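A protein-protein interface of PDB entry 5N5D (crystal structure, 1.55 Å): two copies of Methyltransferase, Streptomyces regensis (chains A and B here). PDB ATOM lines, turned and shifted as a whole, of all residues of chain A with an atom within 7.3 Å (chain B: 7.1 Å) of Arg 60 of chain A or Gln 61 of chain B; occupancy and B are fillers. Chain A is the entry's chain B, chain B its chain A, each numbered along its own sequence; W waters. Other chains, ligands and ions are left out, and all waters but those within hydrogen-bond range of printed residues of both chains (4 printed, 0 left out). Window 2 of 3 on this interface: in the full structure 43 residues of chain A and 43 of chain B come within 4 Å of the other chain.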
ATOM      1  N   HIS A  54     -22.209 -17.509  -2.772  1.00  0.00           N
ATOM      2  CA  HIS A  54     -23.334 -18.189  -3.402  1.00  0.00           C
ATOM      3  C   HIS A  54     -23.165 -19.709  -3.345  1.00  0.00           C
ATOM      4  O   HIS A  54     -24.085 -20.439  -2.955  1.00  0.00           O
ATOM      5  CB  HIS A  54     -23.425 -17.672  -4.841  1.00  0.00           C
ATOM      6  CG  HIS A  54     -24.490 -18.304  -5.685  1.00  0.00           C
ATOM      7  ND1 HIS A  54     -25.810 -17.910  -5.641  1.00  0.00           N
ATOM      8  CD2 HIS A  54     -24.416 -19.265  -6.635  1.00  0.00           C
ATOM      9  CE1 HIS A  54     -26.507 -18.616  -6.514  1.00  0.00           C
ATOM     10  NE2 HIS A  54     -25.684 -19.441  -7.134  1.00  0.00           N
ATOM     11  N   LEU A  55     -21.986 -20.201  -3.732  1.00  0.00           N
ATOM     12  CA  LEU A  55     -21.753 -21.640  -3.773  1.00  0.00           C
ATOM     13  C   LEU A  55     -21.733 -22.244  -2.375  1.00  0.00           C
ATOM     14  O   LEU A  55     -22.241 -23.351  -2.168  1.00  0.00           O
ATOM     15  CB  LEU A  55     -20.449 -21.929  -4.513  1.00  0.00           C
ATOM     16  CG  LEU A  55     -20.475 -21.539  -5.993  1.00  0.00           C
ATOM     17  CD1 LEU A  55     -19.085 -21.632  -6.585  1.00  0.00           C
ATOM     18  CD2 LEU A  55     -21.438 -22.414  -6.771  1.00  0.00           C
ATOM     19  N   LEU A  56     -21.162 -21.533  -1.401  1.00  0.00           N
ATOM     20  CA  LEU A  56     -21.185 -22.029  -0.028  1.00  0.00           C
ATOM     21  C   LEU A  56     -22.613 -22.192   0.472  1.00  0.00           C
ATOM     22  O   LEU A  56     -22.950 -23.200   1.107  1.00  0.00           O
ATOM     23  CB  LEU A  56     -20.404 -21.083   0.886  1.00  0.00           C
ATOM     24  CG  LEU A  56     -18.888 -21.079   0.695  1.00  0.00           C
ATOM     25  CD1 LEU A  56     -18.264 -19.943   1.494  1.00  0.00           C
ATOM     26  CD2 LEU A  56     -18.269 -22.411   1.092  1.00  0.00           C
ATOM     27  N   ALA A  57     -23.463 -21.201   0.209  1.00  0.00           N
ATOM     28  CA  ALA A  57     -24.856 -21.286   0.628  1.00  0.00           C
ATOM     29  C   ALA A  57     -25.547 -22.479  -0.021  1.00  0.00           C
ATOM     30  O   ALA A  57     -26.266 -23.229   0.646  1.00  0.00           O
ATOM     31  CB  ALA A  57     -25.578 -19.983   0.288  1.00  0.00           C
ATOM     32  N   ARG A  58     -25.326 -22.680  -1.325  1.00  0.00           N
ATOM     33  CA  ARG A  58     -25.971 -23.793  -2.016  1.00  0.00           C
ATOM     34  C   ARG A  58     -25.437 -25.143  -1.549  1.00  0.00           C
ATOM     35  O   ARG A  58     -26.198 -26.109  -1.437  1.00  0.00           O
ATOM     36  CB  ARG A  58     -25.794 -23.634  -3.520  1.00  0.00           C
ATOM     37  CG  ARG A  58     -26.557 -22.461  -4.068  1.00  0.00           C
ATOM     38  CD  ARG A  58     -26.314 -22.279  -5.537  1.00  0.00           C
ATOM     39  NE  ARG A  58     -26.967 -23.307  -6.334  1.00  0.00           N
ATOM     40  CZ  ARG A  58     -27.069 -23.254  -7.655  1.00  0.00           C
ATOM     41  NH1 ARG A  58     -26.562 -22.221  -8.312  1.00  0.00           N
ATOM     42  NH2 ARG A  58     -27.683 -24.226  -8.313  1.00  0.00           N
ATOM     43  N   LEU A  59     -24.134 -25.225  -1.274  1.00  0.00           N
ATOM     44  CA  LEU A  59     -23.549 -26.468  -0.782  1.00  0.00           C
ATOM     45  C   LEU A  59     -24.129 -26.856   0.568  1.00  0.00           C
ATOM     46  O   LEU A  59     -24.329 -28.044   0.851  1.00  0.00           O
ATOM     47  CB  LEU A  59     -22.033 -26.323  -0.670  1.00  0.00           C
ATOM     48  CG  LEU A  59     -21.270 -26.478  -1.975  1.00  0.00           C
ATOM     49  CD1 LEU A  59     -19.855 -25.957  -1.803  1.00  0.00           C
ATOM     50  CD2 LEU A  59     -21.270 -27.935  -2.392  1.00  0.00           C
ATOM     51  N   ARG A  60     -24.398 -25.868   1.417  1.00  0.00           N
ATOM     52  CA  ARG A  60     -25.039 -26.062   2.709  1.00  0.00           C
ATOM     53  C   ARG A  60     -26.541 -26.278   2.582  1.00  0.00           C
ATOM     54  O   ARG A  60     -27.179 -26.697   3.554  1.00  0.00           O
ATOM     55  CB  ARG A  60     -24.750 -24.836   3.586  1.00  0.00           C
ATOM     56  CG  ARG A  60     -25.469 -24.753   4.937  1.00  0.00           C
ATOM     57  CD  ARG A  60     -24.943 -25.770   5.938  1.00  0.00           C
ATOM     58  NE  ARG A  60     -25.456 -27.114   5.685  1.00  0.00           N
ATOM     59  CZ  ARG A  60     -25.090 -28.204   6.354  1.00  0.00           C
ATOM     60  NH1 ARG A  60     -24.194 -28.134   7.337  1.00  0.00           N
ATOM     61  NH2 ARG A  60     -25.622 -29.375   6.037  1.00  0.00           N
ATOM     62  N   GLN A  61     -27.104 -26.032   1.399  1.00  0.00           N
ATOM     63  CA  GLN A  61     -28.554 -26.014   1.218  1.00  0.00           C
ATOM     64  C   GLN A  61     -29.199 -25.051   2.212  1.00  0.00           C
ATOM     65  O   GLN A  61     -30.220 -25.352   2.834  1.00  0.00           O
ATOM     66  CB  GLN A  61     -29.151 -27.417   1.355  1.00  0.00           C
ATOM     67  CG  GLN A  61     -28.507 -28.462   0.463  1.00  0.00           C
ATOM     68  CD  GLN A  61     -29.053 -29.854   0.715  1.00  0.00           C
ATOM     69  OE1 GLN A  61     -28.633 -30.540   1.647  1.00  0.00           O
ATOM     70  NE2 GLN A  61     -29.999 -30.276  -0.114  1.00  0.00           N
ATOM     71  N   ALA A  62     -28.585 -23.881   2.358  1.00  0.00           N
ATOM     72  CA  ALA A  62     -29.079 -22.878   3.288  1.00  0.00           C
ATOM     73  C   ALA A  62     -30.470 -22.420   2.887  1.00  0.00           C
ATOM     74  O   ALA A  62     -30.704 -22.043   1.736  1.00  0.00           O
ATOM     75  CB  ALA A  62     -28.130 -21.681   3.323  1.00  0.00           C
ATOM     76  N   ARG A  63     -31.396 -22.462   3.841  1.00  0.00           N
ATOM     77  CA  ARG A  63     -32.732 -21.912   3.653  1.00  0.00           C
ATOM     78  C   ARG A  63     -32.902 -20.553   4.311  1.00  0.00           C
ATOM     79  O   ARG A  63     -33.776 -19.786   3.901  1.00  0.00           O
ATOM     80  CB  ARG A  63     -33.792 -22.856   4.227  1.00  0.00           C
ATOM     81  CG  ARG A  63     -33.772 -24.262   3.667  1.00  0.00           C
ATOM     82  CD  ARG A  63     -34.900 -25.100   4.260  1.00  0.00           C
ATOM     83  NE  ARG A  63     -36.219 -24.536   3.968  1.00  0.00           N
ATOM     84  CZ  ARG A  63     -36.865 -23.670   4.744  1.00  0.00           C
ATOM     85  NH1 ARG A  63     -38.059 -23.221   4.383  1.00  0.00           N
ATOM     86  NH2 ARG A  63     -36.327 -23.241   5.879  1.00  0.00           N
ATOM     87  N   ASP A 138     -28.984 -20.787   8.758  1.00  0.00           N
ATOM     88  CA  ASP A 138     -28.084 -21.809   8.239  1.00  0.00           C
ATOM     89  C   ASP A 138     -26.749 -21.243   7.797  1.00  0.00           C
ATOM     90  O   ASP A 138     -25.800 -22.007   7.607  1.00  0.00           O
ATOM     91  CB  ASP A 138     -28.715 -22.495   7.026  1.00  0.00           C
ATOM     92  CG  ASP A 138     -30.032 -23.139   7.354  1.00  0.00           C
ATOM     93  OD1 ASP A 138     -30.089 -23.899   8.342  1.00  0.00           O
ATOM     94  OD2 ASP A 138     -31.011 -22.863   6.647  1.00  0.00           O
ATOM     95  N   MET A 139     -26.677 -19.933   7.595  1.00  0.00           N
ATOM     96  CA  MET A 139     -25.459 -19.289   7.143  1.00  0.00           C
ATOM     97  C   MET A 139     -25.501 -17.841   7.591  1.00  0.00           C
ATOM     98  O   MET A 139     -26.560 -17.207   7.566  1.00  0.00           O
ATOM     99  CB  MET A 139     -25.318 -19.372   5.622  1.00  0.00           C
ATOM    100  CG  MET A 139     -24.145 -18.589   5.065  1.00  0.00           C
ATOM    101  SD  MET A 139     -23.880 -18.980   3.325  1.00  0.00           S
ATOM    102  CE  MET A 139     -22.411 -18.011   2.982  1.00  0.00           C
ATOM    103  N   ARG A 161     -27.905 -22.676  13.934  1.00  0.00           N
ATOM    104  CA  ARG A 161     -28.044 -24.053  14.373  1.00  0.00           C
ATOM    105  C   ARG A 161     -26.750 -24.808  14.107  1.00  0.00           C
ATOM    106  O   ARG A 161     -25.925 -24.370  13.297  1.00  0.00           O
ATOM    107  CB  ARG A 161     -29.201 -24.742  13.638  1.00  0.00           C
ATOM    108  CG  ARG A 161     -29.087 -24.685  12.113  1.00  0.00           C
ATOM    109  CD  ARG A 161     -30.011 -25.686  11.415  1.00  0.00           C
ATOM    110  NE  ARG A 161     -31.234 -25.064  10.903  1.00  0.00           N
ATOM    111  CZ  ARG A 161     -32.466 -25.300  11.348  1.00  0.00           C
ATOM    112  NH1 ARG A 161     -32.690 -26.159  12.337  1.00  0.00           N
ATOM    113  NH2 ARG A 161     -33.495 -24.672  10.793  1.00  0.00           N
ATOM    114  N   PRO A 162     -26.537 -25.945  14.765  1.00  0.00           N
ATOM    115  CA  PRO A 162     -25.411 -26.803  14.386  1.00  0.00           C
ATOM    116  C   PRO A 162     -25.461 -27.127  12.900  1.00  0.00           C
ATOM    117  O   PRO A 162     -26.520 -27.422  12.340  1.00  0.00           O
ATOM    118  CB  PRO A 162     -25.604 -28.049  15.256  1.00  0.00           C
ATOM    119  CG  PRO A 162     -26.374 -27.565  16.432  1.00  0.00           C
ATOM    120  CD  PRO A 162     -27.295 -26.507  15.898  1.00  0.00           C
ATOM    121  N   GLY A 163     -24.300 -27.052  12.258  1.00  0.00           N
ATOM    122  CA  GLY A 163     -24.190 -27.194  10.829  1.00  0.00           C
ATOM    123  C   GLY A 163     -24.091 -25.875  10.093  1.00  0.00           C
ATOM    124  O   GLY A 163     -23.670 -25.859   8.931  1.00  0.00           O
ATOM    125  N   ALA A 164     -24.442 -24.774  10.743  1.00  0.00           N
ATOM    126  CA  ALA A 164     -24.415 -23.482  10.079  1.00  0.00           C
ATOM    127  C   ALA A 164     -22.994 -23.092   9.698  1.00  0.00           C
ATOM    128  O   ALA A 164     -22.018 -23.446  10.373  1.00  0.00           O
ATOM    129  CB  ALA A 164     -25.016 -22.407  10.978  1.00  0.00           C
ATOM    130  N   VAL A 165     -22.878 -22.350   8.600  1.00  0.00           N
ATOM    131  CA  VAL A 165     -21.601 -21.820   8.139  1.00  0.00           C
ATOM    132  C   VAL A 165     -21.580 -20.317   8.389  1.00  0.00           C
ATOM    133  O   VAL A 165     -22.553 -19.610   8.093  1.00  0.00           O
ATOM    134  CB  VAL A 165     -21.343 -22.155   6.657  1.00  0.00           C
ATOM    135  CG1 VAL A 165     -22.462 -21.644   5.772  1.00  0.00           C
ATOM    136  CG2 VAL A 165     -19.995 -21.592   6.215  1.00  0.00           C
ATOM    137  N   LEU A 223     -17.594 -23.467  10.831  1.00  0.00           N
ATOM    138  CA  LEU A 223     -18.701 -24.412  10.886  1.00  0.00           C
ATOM    139  C   LEU A 223     -19.140 -24.552  12.339  1.00  0.00           C
ATOM    140  O   LEU A 223     -18.331 -24.906  13.204  1.00  0.00           O
ATOM    141  CB  LEU A 223     -18.276 -25.768  10.321  1.00  0.00           C
ATOM    142  CG  LEU A 223     -19.242 -26.926  10.550  1.00  0.00           C
ATOM    143  CD1 LEU A 223     -20.454 -26.781   9.666  1.00  0.00           C
ATOM    144  CD2 LEU A 223     -18.541 -28.253  10.306  1.00  0.00           C
ATOM    145  N   VAL A 224     -20.412 -24.271  12.608  1.00  0.00           N
ATOM    146  CA  VAL A 224     -20.959 -24.462  13.945  1.00  0.00           C
ATOM    147  C   VAL A 224     -21.207 -25.948  14.155  1.00  0.00           C
ATOM    148  O   VAL A 224     -21.873 -26.599  13.341  1.00  0.00           O
ATOM    149  CB  VAL A 224     -22.252 -23.656  14.127  1.00  0.00           C
ATOM    150  CG1 VAL A 224     -22.842 -23.896  15.519  1.00  0.00           C
ATOM    151  CG2 VAL A 224     -22.008 -22.183  13.881  1.00  0.00           C
ATOM    152  N   LEU B  55     -13.773 -28.734   6.076  1.00  0.00           N
ATOM    153  CA  LEU B  55     -15.015 -28.025   6.365  1.00  0.00           C
ATOM    154  C   LEU B  55     -15.976 -28.068   5.182  1.00  0.00           C
ATOM    155  O   LEU B  55     -17.192 -28.188   5.373  1.00  0.00           O
ATOM    156  CB  LEU B  55     -14.711 -26.582   6.763  1.00  0.00           C
ATOM    157  CG  LEU B  55     -13.930 -26.421   8.071  1.00  0.00           C
ATOM    158  CD1 LEU B  55     -13.615 -24.965   8.320  1.00  0.00           C
ATOM    159  CD2 LEU B  55     -14.710 -27.003   9.260  1.00  0.00           C
ATOM    160  N   LEU B  56     -15.460 -27.962   3.956  1.00  0.00           N
ATOM    161  CA  LEU B  56     -16.322 -28.094   2.785  1.00  0.00           C
ATOM    162  C   LEU B  56     -16.994 -29.458   2.748  1.00  0.00           C
ATOM    163  O   LEU B  56     -18.192 -29.558   2.463  1.00  0.00           O
ATOM    164  CB  LEU B  56     -15.516 -27.863   1.509  1.00  0.00           C
ATOM    165  CG  LEU B  56     -15.019 -26.434   1.293  1.00  0.00           C
ATOM    166  CD1 LEU B  56     -14.019 -26.392   0.145  1.00  0.00           C
ATOM    167  CD2 LEU B  56     -16.171 -25.466   1.033  1.00  0.00           C
ATOM    168  N   ALA B  57     -16.241 -30.524   3.026  1.00  0.00           N
ATOM    169  CA  ALA B  57     -16.835 -31.857   3.055  1.00  0.00           C
ATOM    170  C   ALA B  57     -17.919 -31.953   4.121  1.00  0.00           C
ATOM    171  O   ALA B  57     -18.979 -32.550   3.894  1.00  0.00           O
ATOM    172  CB  ALA B  57     -15.748 -32.905   3.298  1.00  0.00           C
ATOM    173  N   ARG B  58     -17.669 -31.386   5.301  1.00  0.00           N
ATOM    174  CA  ARG B  58     -18.657 -31.467   6.373  1.00  0.00           C
ATOM    175  C   ARG B  58     -19.888 -30.624   6.059  1.00  0.00           C
ATOM    176  O   ARG B  58     -21.022 -31.035   6.338  1.00  0.00           O
ATOM    177  CB  ARG B  58     -18.020 -31.040   7.692  1.00  0.00           C
ATOM    178  CG  ARG B  58     -16.972 -32.031   8.185  1.00  0.00           C
ATOM    179  CD  ARG B  58     -16.281 -31.568   9.433  1.00  0.00           C
ATOM    180  NE  ARG B  58     -17.166 -31.538  10.589  1.00  0.00           N
ATOM    181  CZ  ARG B  58     -16.752 -31.294  11.825  1.00  0.00           C
ATOM    182  NH1 ARG B  58     -15.467 -31.063  12.066  1.00  0.00           N
ATOM    183  NH2 ARG B  58     -17.622 -31.283  12.815  1.00  0.00           N
ATOM    184  N   LEU B  59     -19.691 -29.455   5.448  1.00  0.00           N
ATOM    185  CA  LEU B  59     -20.828 -28.626   5.063  1.00  0.00           C
ATOM    186  C   LEU B  59     -21.701 -29.335   4.038  1.00  0.00           C
ATOM    187  O   LEU B  59     -22.929 -29.211   4.064  1.00  0.00           O
ATOM    188  CB  LEU B  59     -20.330 -27.291   4.509  1.00  0.00           C
ATOM    189  CG  LEU B  59     -19.799 -26.316   5.555  1.00  0.00           C
ATOM    190  CD1 LEU B  59     -19.059 -25.191   4.857  1.00  0.00           C
ATOM    191  CD2 LEU B  59     -20.943 -25.772   6.396  1.00  0.00           C
ATOM    192  N   ARG B  60     -21.077 -30.058   3.112  1.00  0.00           N
ATOM    193  CA  ARG B  60     -21.792 -30.865   2.132  1.00  0.00           C
ATOM    194  C   ARG B  60     -22.389 -32.128   2.739  1.00  0.00           C
ATOM    195  O   ARG B  60     -23.217 -32.778   2.090  1.00  0.00           O
ATOM    196  CB  ARG B  60     -20.829 -31.223   0.995  1.00  0.00           C
ATOM    197  CG  ARG B  60     -21.395 -32.091  -0.134  1.00  0.00           C
ATOM    198  CD  ARG B  60     -22.460 -31.367  -0.940  1.00  0.00           C
ATOM    199  NE  ARG B  60     -23.768 -31.397  -0.287  1.00  0.00           N
ATOM    200  CZ  ARG B  60     -24.872 -30.844  -0.780  1.00  0.00           C
ATOM    201  NH1 ARG B  60     -24.853 -30.210  -1.951  1.00  0.00           N
ATOM    202  NH2 ARG B  60     -26.008 -30.930  -0.101  1.00  0.00           N
ATOM    203  N   GLN B  61     -22.020 -32.472   3.975  1.00  0.00           N
ATOM    204  CA  GLN B  61     -22.395 -33.755   4.568  1.00  0.00           C
ATOM    205  C   GLN B  61     -21.999 -34.895   3.635  1.00  0.00           C
ATOM    206  O   GLN B  61     -22.763 -35.838   3.396  1.00  0.00           O
ATOM    207  CB  GLN B  61     -23.885 -33.804   4.899  1.00  0.00           C
ATOM    208  CG  GLN B  61     -24.346 -32.682   5.811  1.00  0.00           C
ATOM    209  CD  GLN B  61     -25.816 -32.777   6.155  1.00  0.00           C
ATOM    210  OE1 GLN B  61     -26.676 -32.739   5.274  1.00  0.00           O
ATOM    211  NE2 GLN B  61     -26.114 -32.912   7.442  1.00  0.00           N
ATOM    212  N   ALA B  62     -20.782 -34.795   3.104  1.00  0.00           N
ATOM    213  CA  ALA B  62     -20.266 -35.788   2.179  1.00  0.00           C
ATOM    214  C   ALA B  62     -20.099 -37.125   2.879  1.00  0.00           C
ATOM    215  O   ALA B  62     -19.532 -37.206   3.974  1.00  0.00           O
ATOM    216  CB  ALA B  62     -18.928 -35.333   1.602  1.00  0.00           C
ATOM    217  N   ARG B  63     -20.590 -38.173   2.231  1.00  0.00           N
ATOM    218  CA  ARG B  63     -20.425 -39.545   2.683  1.00  0.00           C
ATOM    219  C   ARG B  63     -19.412 -40.312   1.855  1.00  0.00           C
ATOM    220  O   ARG B  63     -18.773 -41.227   2.372  1.00  0.00           O
ATOM    221  CB  ARG B  63     -21.776 -40.271   2.635  1.00  0.00           C
ATOM    222  CG  ARG B  63     -21.753 -41.718   3.079  1.00  0.00           C
ATOM    223  CD  ARG B  63     -23.176 -42.286   3.148  1.00  0.00           C
ATOM    224  NE  ARG B  63     -23.183 -43.721   3.427  1.00  0.00           N
ATOM    225  CZ  ARG B  63     -23.236 -44.675   2.503  1.00  0.00           C
ATOM    226  NH1 ARG B  63     -23.289 -44.368   1.211  1.00  0.00           N
ATOM    227  NH2 ARG B  63     -23.237 -45.949   2.872  1.00  0.00           N
ATOM    228  N   ARG B  64     -19.251 -39.960   0.583  1.00  0.00           N
ATOM    229  CA  ARG B  64     -18.255 -40.576  -0.278  1.00  0.00           C
ATOM    230  C   ARG B  64     -17.430 -39.471  -0.916  1.00  0.00           C
ATOM    231  O   ARG B  64     -17.987 -38.554  -1.526  1.00  0.00           O
ATOM    232  CB  ARG B  64     -18.896 -41.439  -1.364  1.00  0.00           C
ATOM    233  CG  ARG B  64     -19.677 -42.639  -0.843  1.00  0.00           C
ATOM    234  CD  ARG B  64     -19.977 -43.614  -1.976  1.00  0.00           C
ATOM    235  NE  ARG B  64     -21.029 -44.567  -1.635  1.00  0.00           N
ATOM    236  CZ  ARG B  64     -20.851 -45.649  -0.884  1.00  0.00           C
ATOM    237  NH1 ARG B  64     -19.657 -45.924  -0.373  1.00  0.00           N
ATOM    238  NH2 ARG B  64     -21.874 -46.457  -0.635  1.00  0.00           N
ATOM    239  N   ALA B  82     -13.669 -35.791   7.855  1.00  0.00           N
ATOM    240  CA  ALA B  82     -14.981 -35.197   7.651  1.00  0.00           C
ATOM    241  C   ALA B  82     -16.075 -36.247   7.507  1.00  0.00           C
ATOM    242  O   ALA B  82     -17.258 -35.896   7.547  1.00  0.00           O
ATOM    243  CB  ALA B  82     -14.967 -34.313   6.405  1.00  0.00           C
ATOM    244  N   PRO B  84     -18.689 -39.492   7.929  1.00  0.00           N
ATOM    245  CA  PRO B  84     -19.418 -40.248   8.941  1.00  0.00           C
ATOM    246  C   PRO B  84     -18.888 -41.667   9.026  1.00  0.00           C
ATOM    247  O   PRO B  84     -18.135 -42.109   8.146  1.00  0.00           O
ATOM    248  CB  PRO B  84     -20.857 -40.227   8.414  1.00  0.00           C
ATOM    249  CG  PRO B  84     -20.673 -40.219   6.942  1.00  0.00           C
ATOM    250  CD  PRO B  84     -19.479 -39.332   6.696  1.00  0.00           C
ATOM    251  N   ASP B 138     -19.915 -37.586  -3.364  1.00  0.00           N
ATOM    252  CA  ASP B 138     -20.448 -36.294  -2.951  1.00  0.00           C
ATOM    253  C   ASP B 138     -19.433 -35.170  -3.084  1.00  0.00           C
ATOM    254  O   ASP B 138     -19.823 -33.999  -3.113  1.00  0.00           O
ATOM    255  CB  ASP B 138     -20.909 -36.365  -1.489  1.00  0.00           C
ATOM    256  CG  ASP B 138     -21.945 -37.439  -1.263  1.00  0.00           C
ATOM    257  OD1 ASP B 138     -22.949 -37.460  -2.003  1.00  0.00           O
ATOM    258  OD2 ASP B 138     -21.757 -38.278  -0.361  1.00  0.00           O
HETATM  259  O   HOH W   1     -25.390 -29.850   2.872  1.00  0.00           O
HETATM  260  O   HOH W   2     -26.293 -32.552   2.247  1.00  0.00           O
HETATM  261  O   HOH W   3     -27.708 -29.706   4.343  1.00  0.00           O
HETATM  262  O   HOH W   4     -24.003 -30.728   9.045  1.00  0.00           O
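Water W3 lies within hydrogen-bond range of NH2 of Arg 60 of chain A (2.7 Å), OE1 of Gln 61 of chain A (3.0 Å) and OE1 of Gln 61 of chain B (3.3 Å).
Water W1 lies within hydrogen-bond range of O of Leu 59 of chain B, O of Leu 59 of chain A, NH2 of Arg 60 of chain A and NH2 of Arg 60 of chain B.
Water W2 lies within hydrogen-bond range of NH2 of Arg 60 of chain B (2.9 Å), OE1 of Gln 61 of chain B (3.1 Å) and OE1 of Gln 61 of chain A (3.1 Å).
Water W4 lies within hydrogen-bond range of NH1 of Arg 60 of chain A and NE2 of Gln 61 of chain B.
Along chain B the printed residues that touch a printed residue of chain A span positions 55 to 61.
Printed residues of chain A that touch a printed residue of chain B: Leu 56, Leu 59, Arg 60, Gln 61, Gly 163, Val 165 and Leu 223.
Hydrophobic or aromatic side chains of chain A that line the printed part of chain B: Leu 56, Leu 59, Val 165 and Leu 223.
Among the printed residues, 11 pairs touch across the chains.
Among the printed residues, no Asp or Glu carboxylate lies within 4 Å of a Lys or Arg side-chain nitrogen of the other chain.
The backbone NH (N) of Gly 163 of chain A sits at hydrogen-bond distance from the backbone carbonyl oxygen (O) of Val 224 of chain A, 2.7 Å away.
The backbone carbonyl oxygen (O) of Gly 163 of chain A sits at hydrogen-bond distance from the guanidinium group (NH1) of Arg 60 of chain A (2.8 Å).
O of Asp 138 of chain A sits at hydrogen-bond distance from N of Val 165 of chain A (3.1 Å).
Leu 56 of chain B touches its own counterpart, Leu 56 of chain A.
Leu 59 of chain A touches its own counterpart, Leu 59 of chain B.
Leu 59 of chain A touches Arg 60 of chain B, and with the chains exchanged Arg 60 of chain A touches Leu 59 of chain B.
Arg 60 of chain A touches Gln 61 of chain B, and with the chains exchanged Gln 61 of chain A touches Arg 60 of chain B.
Positions printed for both chains: 55, 56, 57, 58, 59, 60, 61, 62, 63 and 138.
Of the 11 pairs that touch across the chains among the printed residues, 6 have their exchanged pair printed and touching as well.
The backbone carbonyl oxygen (O) of Leu 59 of chain A lies close to the guanidinium group (NH2) of Arg 60 of chain B (3.5 Å).
The side-chain amide oxygen (OE1) of Gln 61 of chain A is in hydrogen-bond range of the guanidinium group (NH2) of Arg 60 of chain B, 3.2 Å away.
NH2 of Arg 60 of chain A sits close to O of Leu 59 of chain B (3.3 Å).
CD2 of Leu 56 of chain B touches CD2 of Leu 56 of chain A, 3.7 Å away.
Leu 59 of chain A touches Leu 59 of chain B.
Arg 60 of chain A touches Gln 61 of chain B.
Leu 59 of chain B touches Gly 163 of chain A (CD2 to O, 3.7 Å).
CB of Val 165 of chain A touches CD2 of Leu 59 of chain B, 3.6 Å away.
Leu 55 of chain B touches Leu 223 of chain A.
Leu 223 of chain A touches Arg 58 of chain B (CD2 to NE, 3.6 Å).
CD2 of Leu 59 of chain B touches CD1 of Leu 223 of chain A, at 3.5 Å.
Of the printed residues of chain B, Leu 56 of chain A touches Leu 56.
Printed residues of chain B within 4 Å of Leu 59 of chain A: Leu 59 and Arg 60.
Of the printed residues of chain B, Arg 60 of chain A touches Leu 59 (3.3 Å) and Gln 61 (3.4 Å).
Of the printed residues of chain B, Gln 61 of chain A touches Arg 60.
Of the printed residues of chain A, Arg 60 of chain B touches Leu 59 (3.3 Å) and Gln 61 (3.2 Å).
Printed residues of chain A within 4 Å of Gln 61 of chain B: Arg 60 (3.4 Å).
Arg 64 of chain B touches none of the printed residues of chain A.
The nearest printed residue of chain B that does not touch Arg 60 of chain A is Arg 58 of chain B (4.4 Å).
The nearest printed residue of chain B that does not touch Leu 56 of chain A is Leu 59 of chain B (4.7 Å).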
